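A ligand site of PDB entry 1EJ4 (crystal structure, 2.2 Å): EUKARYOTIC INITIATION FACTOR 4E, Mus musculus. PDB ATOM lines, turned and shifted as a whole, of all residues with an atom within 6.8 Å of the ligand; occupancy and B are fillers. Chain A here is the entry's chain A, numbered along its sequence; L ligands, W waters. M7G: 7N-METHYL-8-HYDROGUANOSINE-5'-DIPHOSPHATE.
The guanidinium group (NH1) of Arg 130 lies within salt-bridge range of the side-chain carboxylate (OD1) of Asp 63 (2.8 Å). The side-chain sulfur (SD) of Met 74 lies close to the side-chain amide oxygen (OE1) of Gln 30 (3.7 Å). N of Asn 128 is in hydrogen-bond range of O of Lys 135.
The side-chain carboxylate (OE2) of Glu 76 sits at hydrogen-bond distance from a nitrogen (N2) of the ligand (2.8 Å). The side-chain amino group (NZ) of Lys 132 lies within salt-bridge range of an oxygen (O2B) of the ligand (2.8 Å). An oxygen (O1A) of the ligand is in salt-bridge range of the guanidinium group (NH2) of Arg 130. The backbone NH (N) of Trp 75 lies within hydrogen-bond range of an oxygen (O6) of the ligand, 2.9 Å away. The side-chain amino group of Lys 135 is in salt-bridge range of an oxygen (O2B) of the ligand, at 3.3 Å.
Water W1 bridges an oxygen (O1A) of the ligand (2.7 Å) and the side-chain carboxylate (OD2) of Asp 63 (3.4 Å).
The indole nitrogen (NE1) of Trp 29 sits close to a nitrogen (N9) of the ligand (3.5 Å). Met 74 touches the ligand (CA to O6, 3.2 Å). Hydrophobic or aromatic side chains within 4 Å of the ligand: Trp 29, Met 74 and Trp 75. Of the 20 residues printed, 7 come within 4 Å of the ligand.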
ATOM      1  N   PHE A  21      -1.130 -31.520  21.443  1.00  0.00           N
ATOM      2  CA  PHE A  21      -1.245 -30.204  20.842  1.00  0.00           C
ATOM      3  C   PHE A  21      -0.810 -29.178  21.880  1.00  0.00           C
ATOM      4  O   PHE A  21      -1.168 -29.283  23.052  1.00  0.00           O
ATOM      5  CB  PHE A  21      -2.682 -29.888  20.413  1.00  0.00           C
ATOM      6  CG  PHE A  21      -2.831 -28.518  19.810  1.00  0.00           C
ATOM      7  CD1 PHE A  21      -2.623 -28.315  18.437  1.00  0.00           C
ATOM      8  CD2 PHE A  21      -3.097 -27.414  20.610  1.00  0.00           C
ATOM      9  CE1 PHE A  21      -2.676 -27.048  17.885  1.00  0.00           C
ATOM     10  CE2 PHE A  21      -3.157 -26.152  20.074  1.00  0.00           C
ATOM     11  CZ  PHE A  21      -2.941 -25.961  18.699  1.00  0.00           C
ATOM     12  N   ASN A  23      -0.955 -25.114  22.277  1.00  0.00           N
ATOM     13  CA  ASN A  23      -1.519 -23.850  21.797  1.00  0.00           C
ATOM     14  C   ASN A  23      -0.445 -22.827  21.410  1.00  0.00           C
ATOM     15  O   ASN A  23      -0.239 -21.822  22.088  1.00  0.00           O
ATOM     16  CB  ASN A  23      -2.435 -23.259  22.871  1.00  0.00           C
ATOM     17  CG  ASN A  23      -3.223 -22.063  22.352  1.00  0.00           C
ATOM     18  OD1 ASN A  23      -2.657 -20.996  22.093  1.00  0.00           O
ATOM     19  ND2 ASN A  23      -4.529 -22.255  22.194  1.00  0.00           N
ATOM     20  N   TRP A  29      -2.521 -23.931  12.913  1.00  0.00           N
ATOM     21  CA  TRP A  29      -3.075 -24.872  13.876  1.00  0.00           C
ATOM     22  C   TRP A  29      -2.654 -26.297  13.499  1.00  0.00           C
ATOM     23  O   TRP A  29      -2.289 -27.098  14.360  1.00  0.00           O
ATOM     24  CB  TRP A  29      -4.608 -24.817  13.877  1.00  0.00           C
ATOM     25  CG  TRP A  29      -5.199 -25.749  14.873  1.00  0.00           C
ATOM     26  CD1 TRP A  29      -5.491 -25.474  16.176  1.00  0.00           C
ATOM     27  CD2 TRP A  29      -5.454 -27.148  14.698  1.00  0.00           C
ATOM     28  NE1 TRP A  29      -5.907 -26.614  16.829  1.00  0.00           N
ATOM     29  CE2 TRP A  29      -5.893 -27.658  15.942  1.00  0.00           C
ATOM     30  CE3 TRP A  29      -5.360 -28.027  13.599  1.00  0.00           C
ATOM     31  CZ2 TRP A  29      -6.235 -29.006  16.122  1.00  0.00           C
ATOM     32  CZ3 TRP A  29      -5.697 -29.364  13.785  1.00  0.00           C
ATOM     33  CH2 TRP A  29      -6.121 -29.840  15.034  1.00  0.00           C
ATOM     34  N   GLN A  30      -2.704 -26.592  12.208  1.00  0.00           N
ATOM     35  CA  GLN A  30      -2.381 -27.921  11.730  1.00  0.00           C
ATOM     36  C   GLN A  30      -0.917 -28.334  11.928  1.00  0.00           C
ATOM     37  O   GLN A  30      -0.612 -29.517  12.115  1.00  0.00           O
ATOM     38  CB  GLN A  30      -2.759 -28.020  10.256  1.00  0.00           C
ATOM     39  CG  GLN A  30      -2.780 -29.438   9.727  1.00  0.00           C
ATOM     40  CD  GLN A  30      -3.262 -29.496   8.288  1.00  0.00           C
ATOM     41  OE1 GLN A  30      -4.286 -28.892   7.935  1.00  0.00           O
ATOM     42  NE2 GLN A  30      -2.533 -30.247   7.449  1.00  0.00           N
ATOM     43  N   LEU A  33       0.117 -29.869  15.621  1.00  0.00           N
ATOM     44  CA  LEU A  33      -0.228 -31.219  16.016  1.00  0.00           C
ATOM     45  C   LEU A  33       1.103 -31.962  16.084  1.00  0.00           C
ATOM     46  O   LEU A  33       1.856 -31.987  15.107  1.00  0.00           O
ATOM     47  CB  LEU A  33      -1.133 -31.876  14.976  1.00  0.00           C
ATOM     48  CG  LEU A  33      -2.610 -31.477  14.960  1.00  0.00           C
ATOM     49  CD1 LEU A  33      -2.745 -29.971  14.960  1.00  0.00           C
ATOM     50  CD2 LEU A  33      -3.265 -32.082  13.728  1.00  0.00           C
ATOM     51  N   GLY A  61      -5.091 -24.821  26.826  1.00  0.00           N
ATOM     52  CA  GLY A  61      -4.788 -24.583  25.432  1.00  0.00           C
ATOM     53  C   GLY A  61      -4.136 -25.794  24.779  1.00  0.00           C
ATOM     54  O   GLY A  61      -3.858 -25.795  23.583  1.00  0.00           O
ATOM     55  N   ASP A  63      -4.041 -30.155  24.070  1.00  0.00           N
ATOM     56  CA  ASP A  63      -4.907 -31.316  23.907  1.00  0.00           C
ATOM     57  C   ASP A  63      -4.119 -32.619  23.792  1.00  0.00           C
ATOM     58  O   ASP A  63      -2.898 -32.619  23.606  1.00  0.00           O
ATOM     59  CB  ASP A  63      -5.743 -31.246  22.625  1.00  0.00           C
ATOM     60  CG  ASP A  63      -6.353 -29.895  22.365  1.00  0.00           C
ATOM     61  OD1 ASP A  63      -7.030 -29.332  23.241  1.00  0.00           O
ATOM     62  OD2 ASP A  63      -6.165 -29.392  21.249  1.00  0.00           O
ATOM     63  N   PRO A  73      -5.735 -36.108  13.663  1.00  0.00           N
ATOM     64  CA  PRO A  73      -6.762 -35.519  14.538  1.00  0.00           C
ATOM     65  C   PRO A  73      -7.222 -34.121  14.121  1.00  0.00           C
ATOM     66  O   PRO A  73      -7.160 -33.181  14.919  1.00  0.00           O
ATOM     67  CB  PRO A  73      -6.080 -35.549  15.906  1.00  0.00           C
ATOM     68  CG  PRO A  73      -4.645 -35.287  15.545  1.00  0.00           C
ATOM     69  CD  PRO A  73      -4.485 -36.297  14.417  1.00  0.00           C
ATOM     70  N   MET A  74      -7.709 -34.008  12.889  1.00  0.00           N
ATOM     71  CA  MET A  74      -8.158 -32.729  12.371  1.00  0.00           C
ATOM     72  C   MET A  74      -9.348 -32.870  11.425  1.00  0.00           C
ATOM     73  O   MET A  74      -9.558 -33.925  10.827  1.00  0.00           O
ATOM     74  CB  MET A  74      -6.982 -32.040  11.651  1.00  0.00           C
ATOM     75  CG  MET A  74      -6.447 -32.825  10.475  1.00  0.00           C
ATOM     76  SD  MET A  74      -4.995 -32.061   9.687  1.00  0.00           S
ATOM     77  CE  MET A  74      -4.793 -33.172   8.253  1.00  0.00           C
ATOM     78  N   TRP A  75     -10.142 -31.807  11.279  1.00  0.00           N
ATOM     79  CA  TRP A  75     -11.331 -31.855  10.418  1.00  0.00           C
ATOM     80  C   TRP A  75     -11.050 -32.172   8.932  1.00  0.00           C
ATOM     81  O   TRP A  75     -11.804 -32.919   8.301  1.00  0.00           O
ATOM     82  CB  TRP A  75     -12.106 -30.524  10.489  1.00  0.00           C
ATOM     83  CG  TRP A  75     -12.421 -30.003  11.879  1.00  0.00           C
ATOM     84  CD1 TRP A  75     -12.914 -30.715  12.946  1.00  0.00           C
ATOM     85  CD2 TRP A  75     -12.358 -28.635  12.317  1.00  0.00           C
ATOM     86  NE1 TRP A  75     -13.148 -29.886  14.008  1.00  0.00           N
ATOM     87  CE2 TRP A  75     -12.814 -28.604  13.651  1.00  0.00           C
ATOM     88  CE3 TRP A  75     -11.949 -27.436  11.707  1.00  0.00           C
ATOM     89  CZ2 TRP A  75     -12.884 -27.408  14.395  1.00  0.00           C
ATOM     90  CZ3 TRP A  75     -12.014 -26.253  12.436  1.00  0.00           C
ATOM     91  CH2 TRP A  75     -12.479 -26.244  13.772  1.00  0.00           C
ATOM     92  N   GLU A  76      -9.973 -31.608   8.383  1.00  0.00           N
ATOM     93  CA  GLU A  76      -9.616 -31.785   6.971  1.00  0.00           C
ATOM     94  C   GLU A  76      -9.320 -33.204   6.490  1.00  0.00           C
ATOM     95  O   GLU A  76      -9.438 -33.499   5.309  1.00  0.00           O
ATOM     96  CB  GLU A  76      -8.429 -30.883   6.590  1.00  0.00           C
ATOM     97  CG  GLU A  76      -8.658 -29.392   6.782  1.00  0.00           C
ATOM     98  CD  GLU A  76      -8.779 -28.991   8.246  1.00  0.00           C
ATOM     99  OE1 GLU A  76      -9.758 -29.380   8.915  1.00  0.00           O
ATOM    100  OE2 GLU A  76      -7.869 -28.297   8.748  1.00  0.00           O
ATOM    101  N   ARG A  85     -18.692 -35.464  16.200  1.00  0.00           N
ATOM    102  CA  ARG A  85     -18.427 -36.148  17.453  1.00  0.00           C
ATOM    103  C   ARG A  85     -19.445 -35.989  18.573  1.00  0.00           C
ATOM    104  O   ARG A  85     -20.323 -35.128  18.533  1.00  0.00           O
ATOM    105  CB  ARG A  85     -17.070 -35.757  18.002  1.00  0.00           C
ATOM    106  CG  ARG A  85     -16.994 -34.391  18.688  1.00  0.00           C
ATOM    107  CD  ARG A  85     -16.737 -33.276  17.730  1.00  0.00           C
ATOM    108  NE  ARG A  85     -16.060 -32.155  18.390  1.00  0.00           N
ATOM    109  CZ  ARG A  85     -16.621 -31.373  19.291  1.00  0.00           C
ATOM    110  NH1 ARG A  85     -17.879 -31.576  19.655  1.00  0.00           N
ATOM    111  NH2 ARG A  85     -15.920 -30.387  19.857  1.00  0.00           N
ATOM    112  N   VAL A 126     -10.567 -36.925  21.481  1.00  0.00           N
ATOM    113  CA  VAL A 126      -9.830 -35.719  21.854  1.00  0.00           C
ATOM    114  C   VAL A 126     -10.254 -35.181  23.217  1.00  0.00           C
ATOM    115  O   VAL A 126     -11.448 -35.157  23.527  1.00  0.00           O
ATOM    116  CB  VAL A 126     -10.081 -34.552  20.817  1.00  0.00           C
ATOM    117  CG1 VAL A 126      -9.186 -33.362  21.139  1.00  0.00           C
ATOM    118  CG2 VAL A 126      -9.883 -35.026  19.400  1.00  0.00           C
ATOM    119  N   ASN A 128      -9.694 -31.712  25.583  1.00  0.00           N
ATOM    120  CA  ASN A 128      -9.202 -30.342  25.546  1.00  0.00           C
ATOM    121  C   ASN A 128      -9.210 -29.724  26.928  1.00  0.00           C
ATOM    122  O   ASN A 128     -10.244 -29.721  27.594  1.00  0.00           O
ATOM    123  CB  ASN A 128     -10.087 -29.436  24.664  1.00  0.00           C
ATOM    124  CG  ASN A 128     -10.327 -29.981  23.281  1.00  0.00           C
ATOM    125  OD1 ASN A 128     -11.462 -30.319  22.929  1.00  0.00           O
ATOM    126  ND2 ASN A 128      -9.278 -30.079  22.470  1.00  0.00           N
ATOM    127  N   ARG A 130      -8.972 -26.266  28.825  1.00  0.00           N
ATOM    128  CA  ARG A 130      -9.086 -24.846  28.595  1.00  0.00           C
ATOM    129  C   ARG A 130      -9.428 -24.128  29.908  1.00  0.00           C
ATOM    130  O   ARG A 130     -10.149 -24.679  30.749  1.00  0.00           O
ATOM    131  CB  ARG A 130     -10.177 -24.561  27.553  1.00  0.00           C
ATOM    132  CG  ARG A 130      -9.937 -25.169  26.168  1.00  0.00           C
ATOM    133  CD  ARG A 130      -8.699 -24.582  25.525  1.00  0.00           C
ATOM    134  NE  ARG A 130      -8.464 -25.062  24.167  1.00  0.00           N
ATOM    135  CZ  ARG A 130      -7.912 -26.228  23.842  1.00  0.00           C
ATOM    136  NH1 ARG A 130      -7.506 -27.076  24.783  1.00  0.00           N
ATOM    137  NH2 ARG A 130      -7.777 -26.551  22.561  1.00  0.00           N
ATOM    138  N   LYS A 132     -11.459 -22.033  30.442  1.00  0.00           N
ATOM    139  CA  LYS A 132     -12.918 -21.864  30.539  1.00  0.00           C
ATOM    140  C   LYS A 132     -13.703 -23.150  30.802  1.00  0.00           C
ATOM    141  O   LYS A 132     -14.883 -23.110  31.117  1.00  0.00           O
ATOM    142  CB  LYS A 132     -13.447 -21.223  29.252  1.00  0.00           C
ATOM    143  CG  LYS A 132     -13.130 -22.036  28.007  1.00  0.00           C
ATOM    144  CD  LYS A 132     -13.774 -21.428  26.771  1.00  0.00           C
ATOM    145  CE  LYS A 132     -13.448 -22.242  25.504  1.00  0.00           C
ATOM    146  NZ  LYS A 132     -12.006 -22.177  25.158  1.00  0.00           N
ATOM    147  N   GLY A 133     -13.042 -24.296  30.660  1.00  0.00           N
ATOM    148  CA  GLY A 133     -13.711 -25.572  30.864  1.00  0.00           C
ATOM    149  C   GLY A 133     -13.016 -26.598  29.996  1.00  0.00           C
ATOM    150  O   GLY A 133     -12.285 -26.211  29.090  1.00  0.00           O
ATOM    151  N   LYS A 135     -12.998 -30.368  27.615  1.00  0.00           N
ATOM    152  CA  LYS A 135     -13.840 -31.148  26.725  1.00  0.00           C
ATOM    153  C   LYS A 135     -13.244 -32.491  26.344  1.00  0.00           C
ATOM    154  O   LYS A 135     -12.033 -32.645  26.240  1.00  0.00           O
ATOM    155  CB  LYS A 135     -14.130 -30.353  25.453  1.00  0.00           C
ATOM    156  CG  LYS A 135     -15.120 -29.210  25.612  1.00  0.00           C
ATOM    157  CD  LYS A 135     -15.246 -28.378  24.317  1.00  0.00           C
ATOM    158  CE  LYS A 135     -13.929 -27.669  24.005  1.00  0.00           C
ATOM    159  NZ  LYS A 135     -14.008 -26.751  22.831  1.00  0.00           N
ATOM    160  N   TRP A 139     -14.770 -38.804  17.923  1.00  0.00           N
ATOM    161  CA  TRP A 139     -14.980 -38.449  16.529  1.00  0.00           C
ATOM    162  C   TRP A 139     -15.388 -39.664  15.681  1.00  0.00           C
ATOM    163  O   TRP A 139     -14.737 -40.708  15.747  1.00  0.00           O
ATOM    164  CB  TRP A 139     -13.674 -37.876  15.963  1.00  0.00           C
ATOM    165  CG  TRP A 139     -13.322 -36.500  16.460  1.00  0.00           C
ATOM    166  CD1 TRP A 139     -13.556 -35.993  17.688  1.00  0.00           C
ATOM    167  CD2 TRP A 139     -12.596 -35.490  15.743  1.00  0.00           C
ATOM    168  NE1 TRP A 139     -13.017 -34.739  17.803  1.00  0.00           N
ATOM    169  CE2 TRP A 139     -12.425 -34.405  16.611  1.00  0.00           C
ATOM    170  CE3 TRP A 139     -12.076 -35.409  14.434  1.00  0.00           C
ATOM    171  CZ2 TRP A 139     -11.744 -33.225  16.235  1.00  0.00           C
ATOM    172  CZ3 TRP A 139     -11.393 -34.235  14.051  1.00  0.00           C
ATOM    173  CH2 TRP A 139     -11.230 -33.166  14.955  1.00  0.00           C
ATOM    174  N   THR A 176     -19.344 -27.076  13.829  1.00  0.00           N
ATOM    175  CA  THR A 176     -18.330 -26.600  14.761  1.00  0.00           C
ATOM    176  C   THR A 176     -17.328 -25.687  14.050  1.00  0.00           C
ATOM    177  O   THR A 176     -16.844 -24.729  14.639  1.00  0.00           O
ATOM    178  CB  THR A 176     -17.529 -27.771  15.386  1.00  0.00           C
ATOM    179  OG1 THR A 176     -18.429 -28.727  15.955  1.00  0.00           O
ATOM    180  CG2 THR A 176     -16.608 -27.248  16.459  1.00  0.00           C
HETATM  181  PA  M7G L   1     -10.627 -25.796  19.778  1.00  0.00           P
HETATM  182  O1A M7G L   1      -9.220 -26.117  20.147  1.00  0.00           O
HETATM  183  O2A M7G L   1     -11.219 -26.992  19.142  1.00  0.00           O
HETATM  184  O3A M7G L   1     -11.475 -25.424  21.109  1.00  0.00           O
HETATM  185  O5' M7G L   1     -10.659 -24.538  18.759  1.00  0.00           O
HETATM  186  PB  M7G L   1     -11.379 -23.990  21.813  1.00  0.00           P
HETATM  187  O1B M7G L   1      -9.958 -23.699  22.132  1.00  0.00           O
HETATM  188  O2B M7G L   1     -12.183 -24.033  23.054  1.00  0.00           O
HETATM  189  O3B M7G L   1     -11.936 -22.954  20.891  1.00  0.00           O
HETATM  190  C5' M7G L   1      -9.577 -23.638  18.636  1.00  0.00           C
HETATM  191  C4' M7G L   1      -9.302 -23.184  17.245  1.00  0.00           C
HETATM  192  O4' M7G L   1      -8.418 -24.171  16.706  1.00  0.00           O
HETATM  193  C3' M7G L   1     -10.430 -23.301  16.261  1.00  0.00           C
HETATM  194  O3' M7G L   1     -11.277 -22.134  16.279  1.00  0.00           O
HETATM  195  C2' M7G L   1      -9.670 -23.327  14.912  1.00  0.00           C
HETATM  196  O2' M7G L   1      -9.117 -21.988  14.589  1.00  0.00           O
HETATM  197  C1' M7G L   1      -8.589 -24.322  15.282  1.00  0.00           C
HETATM  198  N9  M7G L   1      -8.897 -25.773  15.251  1.00  0.00           N
HETATM  199  C8  M7G L   1      -9.327 -26.676  16.175  1.00  0.00           C
HETATM  200  N7  M7G L   1      -9.436 -27.847  15.613  1.00  0.00           N
HETATM  201  CM7 M7G L   1      -9.883 -29.065  16.292  1.00  0.00           C
HETATM  202  C5  M7G L   1      -9.076 -27.799  14.127  1.00  0.00           C
HETATM  203  C6  M7G L   1      -9.007 -28.618  13.117  1.00  0.00           C
HETATM  204  O6  M7G L   1      -9.306 -29.837  13.168  1.00  0.00           O
HETATM  205  N1  M7G L   1      -8.569 -27.980  11.929  1.00  0.00           N
HETATM  206  C2  M7G L   1      -8.232 -26.648  11.800  1.00  0.00           C
HETATM  207  N2  M7G L   1      -7.841 -26.215  10.628  1.00  0.00           N
HETATM  208  N3  M7G L   1      -8.298 -25.789  12.846  1.00  0.00           N
HETATM  209  C4  M7G L   1      -8.730 -26.398  14.039  1.00  0.00           C
HETATM  210  O   HOH W   1      -8.757 -28.589  19.137  1.00  0.00           O
